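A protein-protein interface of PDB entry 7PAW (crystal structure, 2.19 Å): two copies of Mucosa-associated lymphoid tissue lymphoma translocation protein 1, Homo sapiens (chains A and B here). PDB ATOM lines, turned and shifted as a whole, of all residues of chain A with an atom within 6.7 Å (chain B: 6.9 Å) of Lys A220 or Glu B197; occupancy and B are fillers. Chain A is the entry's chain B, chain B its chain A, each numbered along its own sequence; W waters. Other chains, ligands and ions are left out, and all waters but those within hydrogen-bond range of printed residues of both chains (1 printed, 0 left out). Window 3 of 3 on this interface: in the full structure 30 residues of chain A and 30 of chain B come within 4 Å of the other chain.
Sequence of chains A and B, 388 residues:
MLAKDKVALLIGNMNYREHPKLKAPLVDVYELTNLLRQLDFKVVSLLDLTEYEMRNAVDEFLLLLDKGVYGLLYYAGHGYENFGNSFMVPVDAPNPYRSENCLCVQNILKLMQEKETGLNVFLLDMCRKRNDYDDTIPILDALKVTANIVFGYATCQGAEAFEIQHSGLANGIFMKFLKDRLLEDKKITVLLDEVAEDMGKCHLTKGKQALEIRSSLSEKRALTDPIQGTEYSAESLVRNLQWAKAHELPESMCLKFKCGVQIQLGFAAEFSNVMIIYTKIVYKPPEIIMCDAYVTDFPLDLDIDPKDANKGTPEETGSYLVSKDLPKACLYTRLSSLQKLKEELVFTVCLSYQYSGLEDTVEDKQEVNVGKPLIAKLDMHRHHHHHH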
ATOM      1  N   MET A   1      17.997  36.188   7.341  1.00  0.00           N
ATOM      2  CA  MET A   1      17.619  37.273   6.437  1.00  0.00           C
ATOM      3  C   MET A   1      16.618  38.245   7.096  1.00  0.00           C
ATOM      4  O   MET A   1      16.048  37.936   8.151  1.00  0.00           O
ATOM      5  CB  MET A   1      17.027  36.720   5.126  1.00  0.00           C
ATOM      6  CG  MET A   1      17.875  35.681   4.442  1.00  0.00           C
ATOM      7  SD  MET A   1      19.403  36.319   3.759  1.00  0.00           S
ATOM      8  CE  MET A   1      18.875  36.750   2.158  1.00  0.00           C
ATOM      9  N   TYR A  70       7.874  40.510   2.559  1.00  0.00           N
ATOM     10  CA  TYR A  70       7.555  39.088   2.458  1.00  0.00           C
ATOM     11  C   TYR A  70       6.052  39.019   2.269  1.00  0.00           C
ATOM     12  O   TYR A  70       5.292  39.488   3.119  1.00  0.00           O
ATOM     13  CB  TYR A  70       7.943  38.338   3.733  1.00  0.00           C
ATOM     14  CG  TYR A  70       9.405  37.977   3.869  1.00  0.00           C
ATOM     15  CD1 TYR A  70      10.401  38.798   3.344  1.00  0.00           C
ATOM     16  CD2 TYR A  70       9.799  36.863   4.603  1.00  0.00           C
ATOM     17  CE1 TYR A  70      11.746  38.485   3.492  1.00  0.00           C
ATOM     18  CE2 TYR A  70      11.143  36.526   4.736  1.00  0.00           C
ATOM     19  CZ  TYR A  70      12.113  37.351   4.194  1.00  0.00           C
ATOM     20  OH  TYR A  70      13.435  37.059   4.380  1.00  0.00           O
ATOM     21  N   LYS A 187      14.077  27.432   6.536  1.00  0.00           N
ATOM     22  CA  LYS A 187      13.908  28.015   5.201  1.00  0.00           C
ATOM     23  C   LYS A 187      12.570  27.446   4.653  1.00  0.00           C
ATOM     24  O   LYS A 187      12.315  26.251   4.824  1.00  0.00           O
ATOM     25  CB  LYS A 187      15.129  27.615   4.342  1.00  0.00           C
ATOM     26  CG  LYS A 187      15.162  28.150   2.918  1.00  0.00           C
ATOM     27  CD  LYS A 187      16.416  27.703   2.184  1.00  0.00           C
ATOM     28  CE  LYS A 187      16.389  28.152   0.735  1.00  0.00           C
ATOM     29  NZ  LYS A 187      17.575  27.695  -0.030  1.00  0.00           N
ATOM     30  N   ILE A 188      11.693  28.306   4.082  1.00  0.00           N
ATOM     31  CA  ILE A 188      10.320  27.961   3.650  1.00  0.00           C
ATOM     32  C   ILE A 188      10.278  26.743   2.722  1.00  0.00           C
ATOM     33  O   ILE A 188       9.330  25.971   2.807  1.00  0.00           O
ATOM     34  CB  ILE A 188       9.543  29.193   3.080  1.00  0.00           C
ATOM     35  CG1 ILE A 188       8.024  28.922   2.843  1.00  0.00           C
ATOM     36  CG2 ILE A 188      10.206  29.770   1.806  1.00  0.00           C
ATOM     37  CD1 ILE A 188       7.177  28.394   4.021  1.00  0.00           C
ATOM     38  N   LEU A 217      13.659  30.063  -5.067  1.00  0.00           N
ATOM     39  CA  LEU A 217      14.307  30.727  -3.935  1.00  0.00           C
ATOM     40  C   LEU A 217      15.792  30.370  -3.874  1.00  0.00           C
ATOM     41  O   LEU A 217      16.160  29.211  -3.702  1.00  0.00           O
ATOM     42  CB  LEU A 217      13.580  30.381  -2.614  1.00  0.00           C
ATOM     43  CG  LEU A 217      14.062  31.065  -1.315  1.00  0.00           C
ATOM     44  CD1 LEU A 217      13.805  32.557  -1.338  1.00  0.00           C
ATOM     45  CD2 LEU A 217      13.421  30.435  -0.080  1.00  0.00           C
ATOM     46  N   SER A 218      16.642  31.376  -4.054  1.00  0.00           N
ATOM     47  CA  SER A 218      18.095  31.213  -4.075  1.00  0.00           C
ATOM     48  C   SER A 218      18.729  31.778  -2.807  1.00  0.00           C
ATOM     49  O   SER A 218      19.931  32.010  -2.795  1.00  0.00           O
ATOM     50  CB  SER A 218      18.662  31.915  -5.300  1.00  0.00           C
ATOM     51  OG  SER A 218      18.300  33.285  -5.282  1.00  0.00           O
ATOM     52  N   GLU A 219      17.923  32.027  -1.753  1.00  0.00           N
ATOM     53  CA  GLU A 219      18.399  32.600  -0.494  1.00  0.00           C
ATOM     54  C   GLU A 219      17.753  31.897   0.709  1.00  0.00           C
ATOM     55  O   GLU A 219      16.655  31.373   0.570  1.00  0.00           O
ATOM     56  CB  GLU A 219      18.071  34.110  -0.440  1.00  0.00           C
ATOM     57  CG  GLU A 219      18.879  34.985  -1.386  1.00  0.00           C
ATOM     58  CD  GLU A 219      18.539  36.464  -1.362  1.00  0.00           C
ATOM     59  OE1 GLU A 219      19.449  37.280  -1.632  1.00  0.00           O
ATOM     60  OE2 GLU A 219      17.372  36.809  -1.064  1.00  0.00           O
ATOM     61  N   LYS A 220      18.420  31.917   1.892  1.00  0.00           N
ATOM     62  CA  LYS A 220      17.923  31.306   3.134  1.00  0.00           C
ATOM     63  C   LYS A 220      16.816  32.172   3.719  1.00  0.00           C
ATOM     64  O   LYS A 220      17.029  32.845   4.727  1.00  0.00           O
ATOM     65  CB  LYS A 220      19.058  31.155   4.161  1.00  0.00           C
ATOM     66  CG  LYS A 220      19.541  29.738   4.427  1.00  0.00           C
ATOM     67  CD  LYS A 220      20.558  29.742   5.575  1.00  0.00           C
ATOM     68  CE  LYS A 220      21.921  29.190   5.202  1.00  0.00           C
ATOM     69  NZ  LYS A 220      22.749  30.169   4.442  1.00  0.00           N
ATOM     70  N   ARG A 221      15.630  32.156   3.105  1.00  0.00           N
ATOM     71  CA  ARG A 221      14.511  32.948   3.605  1.00  0.00           C
ATOM     72  C   ARG A 221      13.459  32.083   4.264  1.00  0.00           C
ATOM     73  O   ARG A 221      13.094  31.039   3.742  1.00  0.00           O
ATOM     74  CB  ARG A 221      13.926  33.878   2.529  1.00  0.00           C
ATOM     75  CG  ARG A 221      14.919  34.970   2.159  1.00  0.00           C
ATOM     76  CD  ARG A 221      14.292  36.093   1.382  1.00  0.00           C
ATOM     77  NE  ARG A 221      15.291  37.053   0.904  1.00  0.00           N
ATOM     78  CZ  ARG A 221      15.684  38.135   1.568  1.00  0.00           C
ATOM     79  NH1 ARG A 221      15.161  38.422   2.751  1.00  0.00           N
ATOM     80  NH2 ARG A 221      16.612  38.933   1.055  1.00  0.00           N
ATOM     81  N   ALA A 222      13.020  32.503   5.443  1.00  0.00           N
ATOM     82  CA  ALA A 222      12.007  31.831   6.259  1.00  0.00           C
ATOM     83  C   ALA A 222      10.879  32.790   6.636  1.00  0.00           C
ATOM     84  O   ALA A 222      11.086  34.006   6.672  1.00  0.00           O
ATOM     85  CB  ALA A 222      12.654  31.281   7.522  1.00  0.00           C
ATOM     86  N   ASP A 225      11.668  35.149   9.684  1.00  0.00           N
ATOM     87  CA  ASP A 225      12.612  36.256   9.524  1.00  0.00           C
ATOM     88  C   ASP A 225      12.113  37.542  10.203  1.00  0.00           C
ATOM     89  O   ASP A 225      10.939  37.882  10.045  1.00  0.00           O
ATOM     90  CB  ASP A 225      12.971  36.466   8.045  1.00  0.00           C
ATOM     91  CG  ASP A 225      13.800  35.328   7.444  1.00  0.00           C
ATOM     92  OD1 ASP A 225      14.377  34.521   8.226  1.00  0.00           O
ATOM     93  OD2 ASP A 225      13.870  35.237   6.204  1.00  0.00           O
ATOM     94  N   PHE B 177      27.920  24.178 -10.278  1.00  0.00           N
ATOM     95  CA  PHE B 177      27.365  24.196  -8.929  1.00  0.00           C
ATOM     96  C   PHE B 177      26.927  22.825  -8.427  1.00  0.00           C
ATOM     97  O   PHE B 177      27.073  22.537  -7.233  1.00  0.00           O
ATOM     98  CB  PHE B 177      26.223  25.220  -8.834  1.00  0.00           C
ATOM     99  CG  PHE B 177      26.725  26.637  -8.965  1.00  0.00           C
ATOM    100  CD1 PHE B 177      27.147  27.349  -7.845  1.00  0.00           C
ATOM    101  CD2 PHE B 177      26.832  27.242 -10.213  1.00  0.00           C
ATOM    102  CE1 PHE B 177      27.643  28.647  -7.973  1.00  0.00           C
ATOM    103  CE2 PHE B 177      27.343  28.535 -10.340  1.00  0.00           C
ATOM    104  CZ  PHE B 177      27.745  29.226  -9.222  1.00  0.00           C
ATOM    105  N   ARG B 181      28.138  19.668  -4.852  1.00  0.00           N
ATOM    106  CA  ARG B 181      27.144  19.241  -3.879  1.00  0.00           C
ATOM    107  C   ARG B 181      26.598  17.825  -4.062  1.00  0.00           C
ATOM    108  O   ARG B 181      26.187  17.215  -3.077  1.00  0.00           O
ATOM    109  CB  ARG B 181      25.990  20.253  -3.850  1.00  0.00           C
ATOM    110  CG  ARG B 181      26.367  21.625  -3.309  1.00  0.00           C
ATOM    111  CD  ARG B 181      26.272  21.666  -1.802  1.00  0.00           C
ATOM    112  NE  ARG B 181      26.104  23.028  -1.302  1.00  0.00           N
ATOM    113  CZ  ARG B 181      25.914  23.333  -0.022  1.00  0.00           C
ATOM    114  NH1 ARG B 181      25.870  22.376   0.898  1.00  0.00           N
ATOM    115  NH2 ARG B 181      25.767  24.598   0.351  1.00  0.00           N
ATOM    116  N   LEU B 192      19.437  19.924  -3.856  1.00  0.00           N
ATOM    117  CA  LEU B 192      19.184  20.811  -4.988  1.00  0.00           C
ATOM    118  C   LEU B 192      18.881  22.240  -4.526  1.00  0.00           C
ATOM    119  O   LEU B 192      19.334  23.194  -5.166  1.00  0.00           O
ATOM    120  CB  LEU B 192      18.065  20.254  -5.900  1.00  0.00           C
ATOM    121  CG  LEU B 192      18.391  18.990  -6.723  1.00  0.00           C
ATOM    122  CD1 LEU B 192      17.239  18.589  -7.605  1.00  0.00           C
ATOM    123  CD2 LEU B 192      19.600  19.183  -7.557  1.00  0.00           C
ATOM    124  N   ASP B 193      18.149  22.383  -3.394  1.00  0.00           N
ATOM    125  CA  ASP B 193      17.805  23.662  -2.770  1.00  0.00           C
ATOM    126  C   ASP B 193      19.060  24.386  -2.287  1.00  0.00           C
ATOM    127  O   ASP B 193      19.131  25.611  -2.371  1.00  0.00           O
ATOM    128  CB  ASP B 193      16.807  23.450  -1.626  1.00  0.00           C
ATOM    129  CG  ASP B 193      16.413  24.704  -0.862  1.00  0.00           C
ATOM    130  OD1 ASP B 193      15.751  25.590  -1.465  1.00  0.00           O
ATOM    131  OD2 ASP B 193      16.756  24.797   0.336  1.00  0.00           O
ATOM    132  N   GLU B 194      20.048  23.633  -1.807  1.00  0.00           N
ATOM    133  CA  GLU B 194      21.355  24.153  -1.398  1.00  0.00           C
ATOM    134  C   GLU B 194      22.162  24.628  -2.611  1.00  0.00           C
ATOM    135  O   GLU B 194      22.775  25.689  -2.536  1.00  0.00           O
ATOM    136  CB  GLU B 194      22.117  23.113  -0.566  1.00  0.00           C
ATOM    137  CG  GLU B 194      21.603  23.074   0.872  1.00  0.00           C
ATOM    138  CD  GLU B 194      22.247  22.075   1.815  1.00  0.00           C
ATOM    139  OE1 GLU B 194      23.269  21.457   1.436  1.00  0.00           O
ATOM    140  OE2 GLU B 194      21.733  21.919   2.946  1.00  0.00           O
ATOM    141  N   VAL B 195      22.091  23.893  -3.753  1.00  0.00           N
ATOM    142  CA  VAL B 195      22.719  24.237  -5.056  1.00  0.00           C
ATOM    143  C   VAL B 195      22.151  25.581  -5.566  1.00  0.00           C
ATOM    144  O   VAL B 195      22.907  26.415  -6.068  1.00  0.00           O
ATOM    145  CB  VAL B 195      22.577  23.105  -6.116  1.00  0.00           C
ATOM    146  CG1 VAL B 195      23.109  23.534  -7.478  1.00  0.00           C
ATOM    147  CG2 VAL B 195      23.278  21.838  -5.669  1.00  0.00           C
ATOM    148  N   ALA B 196      20.824  25.787  -5.409  1.00  0.00           N
ATOM    149  CA  ALA B 196      20.113  27.015  -5.775  1.00  0.00           C
ATOM    150  C   ALA B 196      20.621  28.207  -4.932  1.00  0.00           C
ATOM    151  O   ALA B 196      20.727  29.320  -5.444  1.00  0.00           O
ATOM    152  CB  ALA B 196      18.612  26.822  -5.569  1.00  0.00           C
ATOM    153  N   GLU B 197      20.963  27.957  -3.660  1.00  0.00           N
ATOM    154  CA  GLU B 197      21.504  28.955  -2.737  1.00  0.00           C
ATOM    155  C   GLU B 197      22.954  29.306  -3.128  1.00  0.00           C
ATOM    156  O   GLU B 197      23.334  30.482  -3.088  1.00  0.00           O
ATOM    157  CB  GLU B 197      21.443  28.435  -1.296  1.00  0.00           C
ATOM    158  CG  GLU B 197      20.848  29.428  -0.324  1.00  0.00           C
ATOM    159  CD  GLU B 197      20.968  29.018   1.127  1.00  0.00           C
ATOM    160  OE1 GLU B 197      21.820  29.600   1.837  1.00  0.00           O
ATOM    161  OE2 GLU B 197      20.213  28.115   1.554  1.00  0.00           O
ATOM    162  N   ASP B 198      23.750  28.285  -3.519  1.00  0.00           N
ATOM    163  CA  ASP B 198      25.131  28.458  -3.992  1.00  0.00           C
ATOM    164  C   ASP B 198      25.145  29.404  -5.185  1.00  0.00           C
ATOM    165  O   ASP B 198      25.972  30.301  -5.206  1.00  0.00           O
ATOM    166  CB  ASP B 198      25.762  27.109  -4.401  1.00  0.00           C
ATOM    167  CG  ASP B 198      26.185  26.223  -3.253  1.00  0.00           C
ATOM    168  OD1 ASP B 198      26.142  26.691  -2.090  1.00  0.00           O
ATOM    169  OD2 ASP B 198      26.569  25.065  -3.513  1.00  0.00           O
ATOM    170  N   MET B 199      24.209  29.229  -6.151  1.00  0.00           N
ATOM    171  CA  MET B 199      24.074  30.086  -7.329  1.00  0.00           C
ATOM    172  C   MET B 199      23.677  31.509  -6.962  1.00  0.00           C
ATOM    173  O   MET B 199      24.146  32.452  -7.595  1.00  0.00           O
ATOM    174  CB  MET B 199      23.078  29.502  -8.325  1.00  0.00           C
ATOM    175  CG  MET B 199      23.716  28.562  -9.296  1.00  0.00           C
ATOM    176  SD  MET B 199      22.579  27.598 -10.326  1.00  0.00           S
ATOM    177  CE  MET B 199      21.817  28.916 -11.290  1.00  0.00           C
ATOM    178  N   GLY B 200      22.845  31.649  -5.931  1.00  0.00           N
ATOM    179  CA  GLY B 200      22.386  32.941  -5.435  1.00  0.00           C
ATOM    180  C   GLY B 200      23.513  33.742  -4.825  1.00  0.00           C
ATOM    181  O   GLY B 200      23.580  34.960  -5.007  1.00  0.00           O
ATOM    182  N   LYS B 201      24.420  33.051  -4.109  1.00  0.00           N
ATOM    183  CA  LYS B 201      25.592  33.657  -3.470  1.00  0.00           C
ATOM    184  C   LYS B 201      26.639  34.102  -4.490  1.00  0.00           C
ATOM    185  O   LYS B 201      27.262  35.152  -4.294  1.00  0.00           O
ATOM    186  CB  LYS B 201      26.198  32.716  -2.418  1.00  0.00           C
ATOM    187  CG  LYS B 201      25.535  32.879  -1.061  1.00  0.00           C
ATOM    188  CD  LYS B 201      26.063  31.901  -0.027  1.00  0.00           C
ATOM    189  CE  LYS B 201      25.601  32.256   1.373  1.00  0.00           C
ATOM    190  NZ  LYS B 201      26.278  33.476   1.910  1.00  0.00           N
ATOM    191  N   CYS B 202      26.805  33.328  -5.588  1.00  0.00           N
ATOM    192  CA  CYS B 202      27.771  33.622  -6.652  1.00  0.00           C
ATOM    193  C   CYS B 202      27.473  34.925  -7.399  1.00  0.00           C
ATOM    194  O   CYS B 202      26.395  35.077  -7.983  1.00  0.00           O
ATOM    195  CB  CYS B 202      27.920  32.448  -7.614  1.00  0.00           C
ATOM    196  SG  CYS B 202      29.422  32.513  -8.635  1.00  0.00           S
ATOM    197  N   LEU B 211      18.201  28.389 -10.501  1.00  0.00           N
ATOM    198  CA  LEU B 211      17.698  27.008 -10.504  1.00  0.00           C
ATOM    199  C   LEU B 211      16.224  26.990 -10.139  1.00  0.00           C
ATOM    200  O   LEU B 211      15.785  27.765  -9.281  1.00  0.00           O
ATOM    201  CB  LEU B 211      18.449  26.187  -9.440  1.00  0.00           C
ATOM    202  CG  LEU B 211      18.940  24.826  -9.846  1.00  0.00           C
ATOM    203  CD1 LEU B 211      20.378  24.727  -9.635  1.00  0.00           C
ATOM    204  CD2 LEU B 211      18.325  23.776  -9.009  1.00  0.00           C
HETATM  205  O   HOH W   1      22.338  32.868  -1.996  1.00  0.00           O
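OD2 of Asp B193 lies within salt-bridge range of NZ of Lys A187 (3.0 Å).
The side-chain carboxylate of Glu B197 lies within salt-bridge range of the side-chain amino group of Lys A187 (3.1 Å).
The side-chain carboxylate (OE1) of Glu B197 lies within salt-bridge range of the side-chain amino group (NZ) of Lys A220, 2.8 Å away.
Of the 11 printed residues of chain A, 4 touch a printed residue of chain B.
Printed residues of chain A that touch a printed residue of chain B: Lys A187, Leu A217, Ser A218 and Lys A220.
Among the printed residues, Asp or Glu carboxylates within 4 Å of a Lys or Arg side-chain nitrogen of the other chain: Lys A187 with Asp B193, Lys A187 with Glu B197 and Lys A220 with Glu B197.
No position is printed for both chains.
Leu A217 touches Ala B196.
O of Ala B196 touches CB of Ser A218, at 3.3 Å.
Glu B197 touches Ser A218 (CA to O, 3.4 Å).
O of Ser A218 touches CA of Gly B200 (3.7 Å).
Of the printed residues of chain B, Lys A220 touches Glu B197.
Of the printed residues of chain A, Glu B197 touches Lys A187, Ser A218 and Lys A220.
Of the printed residues of chain A, Ala B196 touches Leu A217 and Ser A218.
Of the printed residues of chain B, Ser A218 touches Ala B196, Glu B197 and Gly B200.
Ile A188 touches none of the printed residues of chain B.
Water W1 lies within hydrogen-bond range of the backbone carbonyl oxygen (O) of Ser A218 (2.7 Å), the backbone carbonyl oxygen (O) of Glu B197 (2.8 Å) and the backbone NH (N) of Lys B201 (3.0 Å).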
